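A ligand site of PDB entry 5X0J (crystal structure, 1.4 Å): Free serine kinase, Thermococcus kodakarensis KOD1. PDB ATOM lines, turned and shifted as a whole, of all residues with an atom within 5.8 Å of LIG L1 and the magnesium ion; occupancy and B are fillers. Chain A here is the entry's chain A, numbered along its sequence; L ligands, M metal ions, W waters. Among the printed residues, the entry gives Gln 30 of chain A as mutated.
The magnesium ion is bound by an oxygen (O4) of LIG L1, an oxygen (O3) of LG2 L2, the side-chain carboxylate of Asp 69, water W4, water W2 and water W5.
N of His 71 sits at hydrogen-bond distance from O6 of LIG L1, at 3.1 Å.
A ring nitrogen (ND1) of His 71 is in hydrogen-bond range of an oxygen (O6) of LIG L1 (2.7 Å).
An oxygen (O1) of LIG L1 is in hydrogen-bond range of the side-chain amide nitrogen of Gln 30 (2.7 Å).
A nitrogen (N1) of LIG L1 sits at hydrogen-bond distance from the backbone carbonyl oxygen (O) of Val 68, at 2.7 Å.
O3 of LIG L1 sits at hydrogen-bond distance from N of His 225, 2.8 Å away.
A ring nitrogen (ND1) of His 225 sits at hydrogen-bond distance from an oxygen (O3) of LIG L1.
The backbone carbonyl oxygen (O) of Thr 223 lies close to a nitrogen (N1) of LIG L1 (3.4 Å).
A nitrogen (N1) of LIG L1 sits at hydrogen-bond distance from the side-chain hydroxyl (OG1) of Thr 223 (2.8 Å).
O5 of LIG L1 is in salt-bridge range of NZ of Lys 221 (3.3 Å).
A ring nitrogen (ND1) of His 72 sits at hydrogen-bond distance from an oxygen (O5) of LIG L1 (3.0 Å).
The backbone NH (N) of Gly 70 is in hydrogen-bond range of an oxygen (O6) of LIG L1.
An oxygen (O2) of LIG L1 is in hydrogen-bond range of the indole nitrogen of Trp 102.
N of His 71 sits at hydrogen-bond distance from O2 of LG2 L2.
O2 of LG2 L2 sits at hydrogen-bond distance from N of His 72.
ND1 of His 72 sits at hydrogen-bond distance from O2 of LG2 L2 (2.7 Å).
An oxygen (O3) of LG2 L2 lies close to the backbone NH (N) of Gly 70, at 3.5 Å.
An oxygen (O1) of LG2 L2 lies within hydrogen-bond range of the backbone NH (N) of Arg 73 (2.8 Å).
The guanidinium group of Arg 73 is in salt-bridge range of an oxygen (O1) of LG2 L2 (2.8 Å).
Glu 4 touches the magnesium ion (OE2 to MG, 3.9 Å).
NH2 of Arg 73 touches the magnesium ion, 3.9 Å away.
Lys 221 touches the magnesium ion (NZ to MG, 3.95 Å).
Along chain A the residues within 4 Å of the magnesium ion span positions 4 to 221.
Merely in contact with LIG L1: Arg 224 (3.6 Å) and Glu 4 (3.8 Å).
Of the 19 residues printed, 12 come within 4 Å of LIG L1.
Water W2 lies within hydrogen-bond range of OD2 of Asp 69 (2.7 Å), O6 of LG2 L2 (2.8 Å) and NH2 of Arg 73 (3.4 Å).
Water W5 bridges the side-chain carboxylate (OE2) of Glu 4 (2.7 Å) and an oxygen (O2) of LIG L1 (2.9 Å).
Water W1 lies within hydrogen-bond range of O5 of LIG L1 (2.7 Å), N of Lys 221 (2.8 Å), O of Gln 31 (2.9 Å) and NE2 of Gln 30 (3.3 Å).
Water W3 bridges O of His 225 and O2 of LIG L1.
The guanidinium group (NH2) of Arg 73 is in salt-bridge range of the side-chain carboxylate (OD2) of Asp 69, at 3.4 Å.
A ring nitrogen (NE2) of His 71 lies within hydrogen-bond range of the backbone NH (N) of Gln 30, at 3.4 Å.
OE1 of Gln 30 sits at hydrogen-bond distance from N of Thr 223 (3.0 Å).
The side-chain amide oxygen of Gln 30 sits at hydrogen-bond distance from the backbone NH of Thr 222 (3.1 Å).
A ring nitrogen (ND1) of His 225 sits at hydrogen-bond distance from the backbone carbonyl oxygen of Val 68.
The side-chain hydroxyl of Thr 223 sits at hydrogen-bond distance from a ring nitrogen (NE2) of His 29.
NZ of Lys 221 is in salt-bridge range of OE2 of Glu 4, at 2.8 Å.
The side-chain amino group of Lys 221 lies within salt-bridge range of the side-chain carboxylate of Glu 36.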
ATOM      1  N   GLU A   4      -9.553  -9.767 -30.450  1.00  0.00           N
ATOM      2  CA  GLU A   4      -8.224  -9.149 -30.321  1.00  0.00           C
ATOM      3  C   GLU A   4      -7.358  -9.372 -31.549  1.00  0.00           C
ATOM      4  O   GLU A   4      -7.364 -10.445 -32.157  1.00  0.00           O
ATOM      5  CB  GLU A   4      -7.501  -9.692 -29.091  1.00  0.00           C
ATOM      6  CG  GLU A   4      -8.152  -9.275 -27.775  1.00  0.00           C
ATOM      7  CD  GLU A   4      -7.915 -10.236 -26.623  1.00  0.00           C
ATOM      8  OE1 GLU A   4      -7.779 -11.458 -26.850  1.00  0.00           O
ATOM      9  OE2 GLU A   4      -7.960  -9.766 -25.479  1.00  0.00           O
ATOM     10  N   HIS A  29     -12.302  -8.650 -12.887  1.00  0.00           N
ATOM     11  CA  HIS A  29     -11.981  -7.241 -12.749  1.00  0.00           C
ATOM     12  C   HIS A  29     -12.409  -6.328 -13.893  1.00  0.00           C
ATOM     13  O   HIS A  29     -12.144  -5.129 -13.840  1.00  0.00           O
ATOM     14  CB  HIS A  29     -10.490  -7.061 -12.440  1.00  0.00           C
ATOM     15  CG  HIS A  29      -9.564  -7.320 -13.596  1.00  0.00           C
ATOM     16  ND1 HIS A  29      -8.962  -8.545 -13.824  1.00  0.00           N
ATOM     17  CD2 HIS A  29      -9.091  -6.500 -14.565  1.00  0.00           C
ATOM     18  CE1 HIS A  29      -8.166  -8.460 -14.877  1.00  0.00           C
ATOM     19  NE2 HIS A  29      -8.241  -7.237 -15.350  1.00  0.00           N
ATOM     20  N   GLN A  30     -13.094  -6.869 -14.895  1.00  0.00           N
ATOM     21  CA  GLN A  30     -13.558  -6.028 -16.006  1.00  0.00           C
ATOM     22  C   GLN A  30     -14.762  -6.646 -16.718  1.00  0.00           C
ATOM     23  O   GLN A  30     -15.094  -7.809 -16.516  1.00  0.00           O
ATOM     24  CB  GLN A  30     -12.412  -5.628 -16.964  1.00  0.00           C
ATOM     25  CG  GLN A  30     -11.549  -6.742 -17.517  1.00  0.00           C
ATOM     26  CD  GLN A  30     -10.243  -6.279 -18.126  1.00  0.00           C
ATOM     27  OE1 GLN A  30      -9.651  -5.258 -17.718  1.00  0.00           O
ATOM     28  NE2 GLN A  30      -9.734  -7.056 -19.078  1.00  0.00           N
ATOM     29  N   GLN A  31     -15.440  -5.804 -17.493  1.00  0.00           N
ATOM     30  CA  GLN A  31     -16.631  -6.172 -18.261  1.00  0.00           C
ATOM     31  C   GLN A  31     -16.302  -6.977 -19.521  1.00  0.00           C
ATOM     32  O   GLN A  31     -15.139  -7.160 -19.896  1.00  0.00           O
ATOM     33  CB  GLN A  31     -17.387  -4.900 -18.654  1.00  0.00           C
ATOM     34  CG  GLN A  31     -17.969  -4.129 -17.470  1.00  0.00           C
ATOM     35  CD  GLN A  31     -18.510  -2.779 -17.853  1.00  0.00           C
ATOM     36  OE1 GLN A  31     -17.933  -2.064 -18.667  1.00  0.00           O
ATOM     37  NE2 GLN A  31     -19.624  -2.403 -17.257  1.00  0.00           N
ATOM     38  N   LEU A  32     -17.361  -7.474 -20.165  1.00  0.00           N
ATOM     39  CA  LEU A  32     -17.283  -8.341 -21.349  1.00  0.00           C
ATOM     40  C   LEU A  32     -17.648  -7.623 -22.631  1.00  0.00           C
ATOM     41  O   LEU A  32     -18.348  -6.621 -22.601  1.00  0.00           O
ATOM     42  CB  LEU A  32     -18.234  -9.531 -21.179  1.00  0.00           C
ATOM     43  CG  LEU A  32     -18.109 -10.335 -19.879  1.00  0.00           C
ATOM     44  CD1 LEU A  32     -19.037 -11.541 -19.907  1.00  0.00           C
ATOM     45  CD2 LEU A  32     -16.668 -10.776 -19.645  1.00  0.00           C
ATOM     46  N   GLU A  36     -16.841 -11.419 -28.214  1.00  0.00           N
ATOM     47  CA  GLU A  36     -15.765 -12.244 -27.638  1.00  0.00           C
ATOM     48  C   GLU A  36     -16.366 -13.419 -26.855  1.00  0.00           C
ATOM     49  O   GLU A  36     -15.906 -14.555 -26.988  1.00  0.00           O
ATOM     50  CB  GLU A  36     -14.889 -11.367 -26.733  1.00  0.00           C
ATOM     51  CG  GLU A  36     -13.649 -12.008 -26.119  1.00  0.00           C
ATOM     52  CD  GLU A  36     -12.443 -12.084 -27.029  1.00  0.00           C
ATOM     53  OE1 GLU A  36     -11.333 -11.755 -26.557  1.00  0.00           O
ATOM     54  OE2 GLU A  36     -12.620 -12.421 -28.217  1.00  0.00           O
ATOM     55  N   ILE A  67      -9.180 -13.012 -11.757  1.00  0.00           N
ATOM     56  CA  ILE A  67      -9.021 -13.354 -13.170  1.00  0.00           C
ATOM     57  C   ILE A  67      -8.057 -12.348 -13.777  1.00  0.00           C
ATOM     58  O   ILE A  67      -8.389 -11.185 -13.941  1.00  0.00           O
ATOM     59  CB  ILE A  67     -10.366 -13.345 -13.918  1.00  0.00           C
ATOM     60  CG1 ILE A  67     -11.312 -14.393 -13.333  1.00  0.00           C
ATOM     61  CG2 ILE A  67     -10.147 -13.616 -15.403  1.00  0.00           C
ATOM     62  CD1 ILE A  67     -12.729 -14.337 -13.875  1.00  0.00           C
ATOM     63  N   VAL A  68      -6.842 -12.796 -14.097  1.00  0.00           N
ATOM     64  CA  VAL A  68      -5.842 -11.963 -14.757  1.00  0.00           C
ATOM     65  C   VAL A  68      -6.189 -11.877 -16.251  1.00  0.00           C
ATOM     66  O   VAL A  68      -6.226 -10.783 -16.815  1.00  0.00           O
ATOM     67  CB  VAL A  68      -4.433 -12.522 -14.487  1.00  0.00           C
ATOM     68  CG1 VAL A  68      -3.372 -11.773 -15.281  1.00  0.00           C
ATOM     69  CG2 VAL A  68      -4.132 -12.437 -12.989  1.00  0.00           C
ATOM     70  N   ASP A  69      -6.406 -13.038 -16.871  1.00  0.00           N
ATOM     71  CA  ASP A  69      -6.849 -13.133 -18.244  1.00  0.00           C
ATOM     72  C   ASP A  69      -7.798 -14.301 -18.323  1.00  0.00           C
ATOM     73  O   ASP A  69      -7.498 -15.390 -17.815  1.00  0.00           O
ATOM     74  CB  ASP A  69      -5.637 -13.352 -19.163  1.00  0.00           C
ATOM     75  CG  ASP A  69      -6.027 -13.476 -20.629  1.00  0.00           C
ATOM     76  OD1 ASP A  69      -7.030 -12.874 -21.056  1.00  0.00           O
ATOM     77  OD2 ASP A  69      -5.299 -14.198 -21.355  1.00  0.00           O
ATOM     78  N   GLY A  70      -8.963 -14.072 -18.928  1.00  0.00           N
ATOM     79  CA  GLY A  70      -9.987 -15.117 -19.044  1.00  0.00           C
ATOM     80  C   GLY A  70     -11.402 -14.748 -18.665  1.00  0.00           C
ATOM     81  O   GLY A  70     -12.187 -15.627 -18.294  1.00  0.00           O
ATOM     82  N   HIS A  71     -11.776 -13.484 -18.772  1.00  0.00           N
ATOM     83  CA  HIS A  71     -13.143 -13.078 -18.402  1.00  0.00           C
ATOM     84  C   HIS A  71     -14.224 -13.755 -19.221  1.00  0.00           C
ATOM     85  O   HIS A  71     -15.274 -14.121 -18.686  1.00  0.00           O
ATOM     86  CB  HIS A  71     -13.272 -11.574 -18.488  1.00  0.00           C
ATOM     87  CG  HIS A  71     -12.527 -10.876 -17.410  1.00  0.00           C
ATOM     88  ND1 HIS A  71     -11.168 -10.687 -17.460  1.00  0.00           N
ATOM     89  CD2 HIS A  71     -12.928 -10.426 -16.195  1.00  0.00           C
ATOM     90  CE1 HIS A  71     -10.760 -10.103 -16.351  1.00  0.00           C
ATOM     91  NE2 HIS A  71     -11.814  -9.954 -15.570  1.00  0.00           N
ATOM     92  N   HIS A  72     -13.954 -13.930 -20.509  1.00  0.00           N
ATOM     93  CA  HIS A  72     -14.952 -14.483 -21.431  1.00  0.00           C
ATOM     94  C   HIS A  72     -15.022 -15.989 -21.308  1.00  0.00           C
ATOM     95  O   HIS A  72     -16.125 -16.559 -21.298  1.00  0.00           O
ATOM     96  CB  HIS A  72     -14.677 -13.992 -22.846  1.00  0.00           C
ATOM     97  CG  HIS A  72     -14.749 -12.499 -22.960  1.00  0.00           C
ATOM     98  ND1 HIS A  72     -13.708 -11.675 -22.583  1.00  0.00           N
ATOM     99  CD2 HIS A  72     -15.761 -11.687 -23.336  1.00  0.00           C
ATOM    100  CE1 HIS A  72     -14.072 -10.419 -22.768  1.00  0.00           C
ATOM    101  NE2 HIS A  72     -15.296 -10.406 -23.225  1.00  0.00           N
ATOM    102  N   ARG A  73     -13.868 -16.631 -21.183  1.00  0.00           N
ATOM    103  CA  ARG A  73     -13.856 -18.060 -20.865  1.00  0.00           C
ATOM    104  C   ARG A  73     -14.640 -18.320 -19.565  1.00  0.00           C
ATOM    105  O   ARG A  73     -15.480 -19.246 -19.499  1.00  0.00           O
ATOM    106  CB  ARG A  73     -12.444 -18.600 -20.740  1.00  0.00           C
ATOM    107  CG  ARG A  73     -11.797 -18.934 -22.075  1.00  0.00           C
ATOM    108  CD  ARG A  73     -10.294 -19.072 -21.968  1.00  0.00           C
ATOM    109  NE  ARG A  73      -9.647 -17.769 -21.824  1.00  0.00           N
ATOM    110  CZ  ARG A  73      -8.367 -17.581 -21.504  1.00  0.00           C
ATOM    111  NH1 ARG A  73      -7.547 -18.622 -21.300  1.00  0.00           N
ATOM    112  NH2 ARG A  73      -7.881 -16.350 -21.427  1.00  0.00           N
ATOM    113  N   TRP A 102      -5.521  -2.785 -23.867  1.00  0.00           N
ATOM    114  CA  TRP A 102      -6.028  -3.061 -25.192  1.00  0.00           C
ATOM    115  C   TRP A 102      -6.772  -1.813 -25.644  1.00  0.00           C
ATOM    116  O   TRP A 102      -7.554  -1.232 -24.878  1.00  0.00           O
ATOM    117  CB  TRP A 102      -7.008  -4.229 -25.200  1.00  0.00           C
ATOM    118  CG  TRP A 102      -6.419  -5.542 -24.826  1.00  0.00           C
ATOM    119  CD1 TRP A 102      -6.447  -6.137 -23.602  1.00  0.00           C
ATOM    120  CD2 TRP A 102      -5.747  -6.457 -25.697  1.00  0.00           C
ATOM    121  NE1 TRP A 102      -5.829  -7.358 -23.646  1.00  0.00           N
ATOM    122  CE2 TRP A 102      -5.373  -7.571 -24.920  1.00  0.00           C
ATOM    123  CE3 TRP A 102      -5.414  -6.434 -27.052  1.00  0.00           C
ATOM    124  CZ2 TRP A 102      -4.692  -8.663 -25.459  1.00  0.00           C
ATOM    125  CZ3 TRP A 102      -4.720  -7.508 -27.593  1.00  0.00           C
ATOM    126  CH2 TRP A 102      -4.358  -8.612 -26.790  1.00  0.00           C
ATOM    127  N   LYS A 221     -11.489  -5.193 -21.506  1.00  0.00           N
ATOM    128  CA  LYS A 221     -10.141  -5.237 -22.066  1.00  0.00           C
ATOM    129  C   LYS A 221      -9.214  -4.127 -21.556  1.00  0.00           C
ATOM    130  O   LYS A 221      -8.250  -3.737 -22.210  1.00  0.00           O
ATOM    131  CB  LYS A 221     -10.209  -5.234 -23.600  1.00  0.00           C
ATOM    132  CG  LYS A 221     -11.065  -6.341 -24.203  1.00  0.00           C
ATOM    133  CD  LYS A 221     -10.481  -7.710 -23.930  1.00  0.00           C
ATOM    134  CE  LYS A 221     -11.201  -8.766 -24.735  1.00  0.00           C
ATOM    135  NZ  LYS A 221     -10.612 -10.127 -24.525  1.00  0.00           N
ATOM    136  N   THR A 222      -9.510  -3.606 -20.374  1.00  0.00           N
ATOM    137  CA  THR A 222      -8.684  -2.570 -19.770  1.00  0.00           C
ATOM    138  C   THR A 222      -7.261  -3.074 -19.507  1.00  0.00           C
ATOM    139  O   THR A 222      -6.298  -2.374 -19.827  1.00  0.00           O
ATOM    140  CB  THR A 222      -9.346  -2.021 -18.498  1.00  0.00           C
ATOM    141  OG1 THR A 222     -10.521  -1.297 -18.879  1.00  0.00           O
ATOM    142  CG2 THR A 222      -8.405  -1.118 -17.704  1.00  0.00           C
ATOM    143  N   THR A 223      -7.126  -4.266 -18.953  1.00  0.00           N
ATOM    144  CA  THR A 223      -5.814  -4.838 -18.677  1.00  0.00           C
ATOM    145  C   THR A 223      -5.344  -5.745 -19.813  1.00  0.00           C
ATOM    146  O   THR A 223      -6.110  -6.527 -20.360  1.00  0.00           O
ATOM    147  CB  THR A 223      -5.814  -5.675 -17.397  1.00  0.00           C
ATOM    148  OG1 THR A 223      -6.766  -6.736 -17.537  1.00  0.00           O
ATOM    149  CG2 THR A 223      -6.183  -4.840 -16.195  1.00  0.00           C
ATOM    150  N   ARG A 224      -4.075  -5.584 -20.176  1.00  0.00           N
ATOM    151  CA  ARG A 224      -3.404  -6.505 -21.068  1.00  0.00           C
ATOM    152  C   ARG A 224      -2.165  -6.986 -20.328  1.00  0.00           C
ATOM    153  O   ARG A 224      -1.142  -6.308 -20.332  1.00  0.00           O
ATOM    154  CB  ARG A 224      -3.029  -5.849 -22.407  1.00  0.00           C
ATOM    155  CG  ARG A 224      -2.312  -6.775 -23.366  1.00  0.00           C
ATOM    156  CD  ARG A 224      -2.158  -6.187 -24.765  1.00  0.00           C
ATOM    157  NE  ARG A 224      -1.229  -5.067 -24.843  1.00  0.00           N
ATOM    158  CZ  ARG A 224       0.099  -5.165 -24.899  1.00  0.00           C
ATOM    159  NH1 ARG A 224       0.716  -6.328 -24.861  1.00  0.00           N
ATOM    160  NH2 ARG A 224       0.834  -4.055 -24.984  1.00  0.00           N
ATOM    161  N   HIS A 225      -2.262  -8.136 -19.669  1.00  0.00           N
ATOM    162  CA  HIS A 225      -1.160  -8.669 -18.895  1.00  0.00           C
ATOM    163  C   HIS A 225      -0.191  -9.428 -19.771  1.00  0.00           C
ATOM    164  O   HIS A 225      -0.602 -10.189 -20.650  1.00  0.00           O
ATOM    165  CB  HIS A 225      -1.675  -9.592 -17.791  1.00  0.00           C
ATOM    166  CG  HIS A 225      -2.492  -8.896 -16.748  1.00  0.00           C
ATOM    167  ND1 HIS A 225      -3.856  -8.752 -16.843  1.00  0.00           N
ATOM    168  CD2 HIS A 225      -2.124  -8.323 -15.586  1.00  0.00           C
ATOM    169  CE1 HIS A 225      -4.307  -8.117 -15.768  1.00  0.00           C
ATOM    170  NE2 HIS A 225      -3.267  -7.834 -14.998  1.00  0.00           N
HETATM  171  N1  LIG L   1      -7.329  -9.229 -18.792  1.00  0.00           N
HETATM  172  C1  LIG L   1      -7.049  -9.702 -20.184  1.00  0.00           C
HETATM  173  C2  LIG L   1      -7.940  -8.933 -21.157  1.00  0.00           C
HETATM  174  O1  LIG L   1      -9.312  -9.143 -20.801  1.00  0.00           O
HETATM  175  C3  LIG L   1      -5.584  -9.561 -20.502  1.00  0.00           C
HETATM  176  O2  LIG L   1      -5.202  -9.582 -21.688  1.00  0.00           O
HETATM  177  O3  LIG L   1      -4.749  -9.438 -19.587  1.00  0.00           O
HETATM  178  P1  LIG L   1     -10.015 -10.588 -21.021  1.00  0.00           P
HETATM  179  O4  LIG L   1      -9.283 -11.223 -22.188  1.00  0.00           O
HETATM  180  O5  LIG L   1     -11.432 -10.197 -21.321  1.00  0.00           O
HETATM  181  O6  LIG L   1      -9.849 -11.309 -19.702  1.00  0.00           O
HETATM  182  P1  LG2 L   2     -10.902 -14.287 -22.450  1.00  0.00           P
HETATM  183  O1  LG2 L   2     -11.410 -15.639 -21.990  1.00  0.00           O
HETATM  184  O2  LG2 L   2     -11.635 -13.130 -21.782  1.00  0.00           O
HETATM  185  O3  LG2 L   2      -9.401 -14.200 -22.376  1.00  0.00           O
HETATM  186  O4  LG2 L   2     -11.299 -14.154 -23.996  1.00  0.00           O
HETATM  187  C1  LG2 L   2     -11.615 -15.275 -24.812  1.00  0.00           C
HETATM  188  C2  LG2 L   2     -10.412 -16.178 -24.945  1.00  0.00           C
HETATM  189  O5  LG2 L   2     -10.847 -17.476 -25.319  1.00  0.00           O
HETATM  190  C3  LG2 L   2      -9.392 -15.823 -26.050  1.00  0.00           C
HETATM  191  O6  LG2 L   2      -8.088 -15.791 -25.485  1.00  0.00           O
HETATM  192  C4  LG2 L   2      -9.451 -16.939 -27.100  1.00  0.00           C
HETATM  193  O7  LG2 L   2      -8.191 -17.206 -27.714  1.00  0.00           O
HETATM  194  C5  LG2 L   2      -9.913 -18.044 -26.201  1.00  0.00           C
HETATM  195  N1  LG2 L   2     -10.513 -19.228 -26.827  1.00  0.00           N
HETATM  196  C6  LG2 L   2     -11.181 -19.315 -27.996  1.00  0.00           C
HETATM  197  N2  LG2 L   2     -11.619 -20.586 -28.219  1.00  0.00           N
HETATM  198  C7  LG2 L   2     -11.220 -21.308 -27.157  1.00  0.00           C
HETATM  199  C8  LG2 L   2     -11.335 -22.720 -26.747  1.00  0.00           C
HETATM  200  N3  LG2 L   2     -11.983 -23.607 -27.541  1.00  0.00           N
HETATM  201  N4  LG2 L   2     -10.778 -23.066 -25.569  1.00  0.00           N
HETATM  202  C9  LG2 L   2     -10.132 -22.193 -24.765  1.00  0.00           C
HETATM  203  N5  LG2 L   2      -9.983 -20.892 -25.084  1.00  0.00           N
HETATM  204  C10 LG2 L   2     -10.501 -20.418 -26.247  1.00  0.00           C
HETATM  205 MG    MG M   1      -8.106 -12.674 -22.835  1.00  0.00          MG
HETATM  206  O   HOH W   1     -12.449  -7.743 -20.845  1.00  0.00           O
HETATM  207  O   HOH W   2      -6.755 -14.095 -23.665  1.00  0.00           O
HETATM  208  O   HOH W   3      -2.662 -10.400 -22.329  1.00  0.00           O
HETATM  209  O   HOH W   4      -8.964 -12.712 -24.782  1.00  0.00           O
HETATM  210  O   HOH W   5      -6.700 -11.222 -23.546  1.00  0.00           O
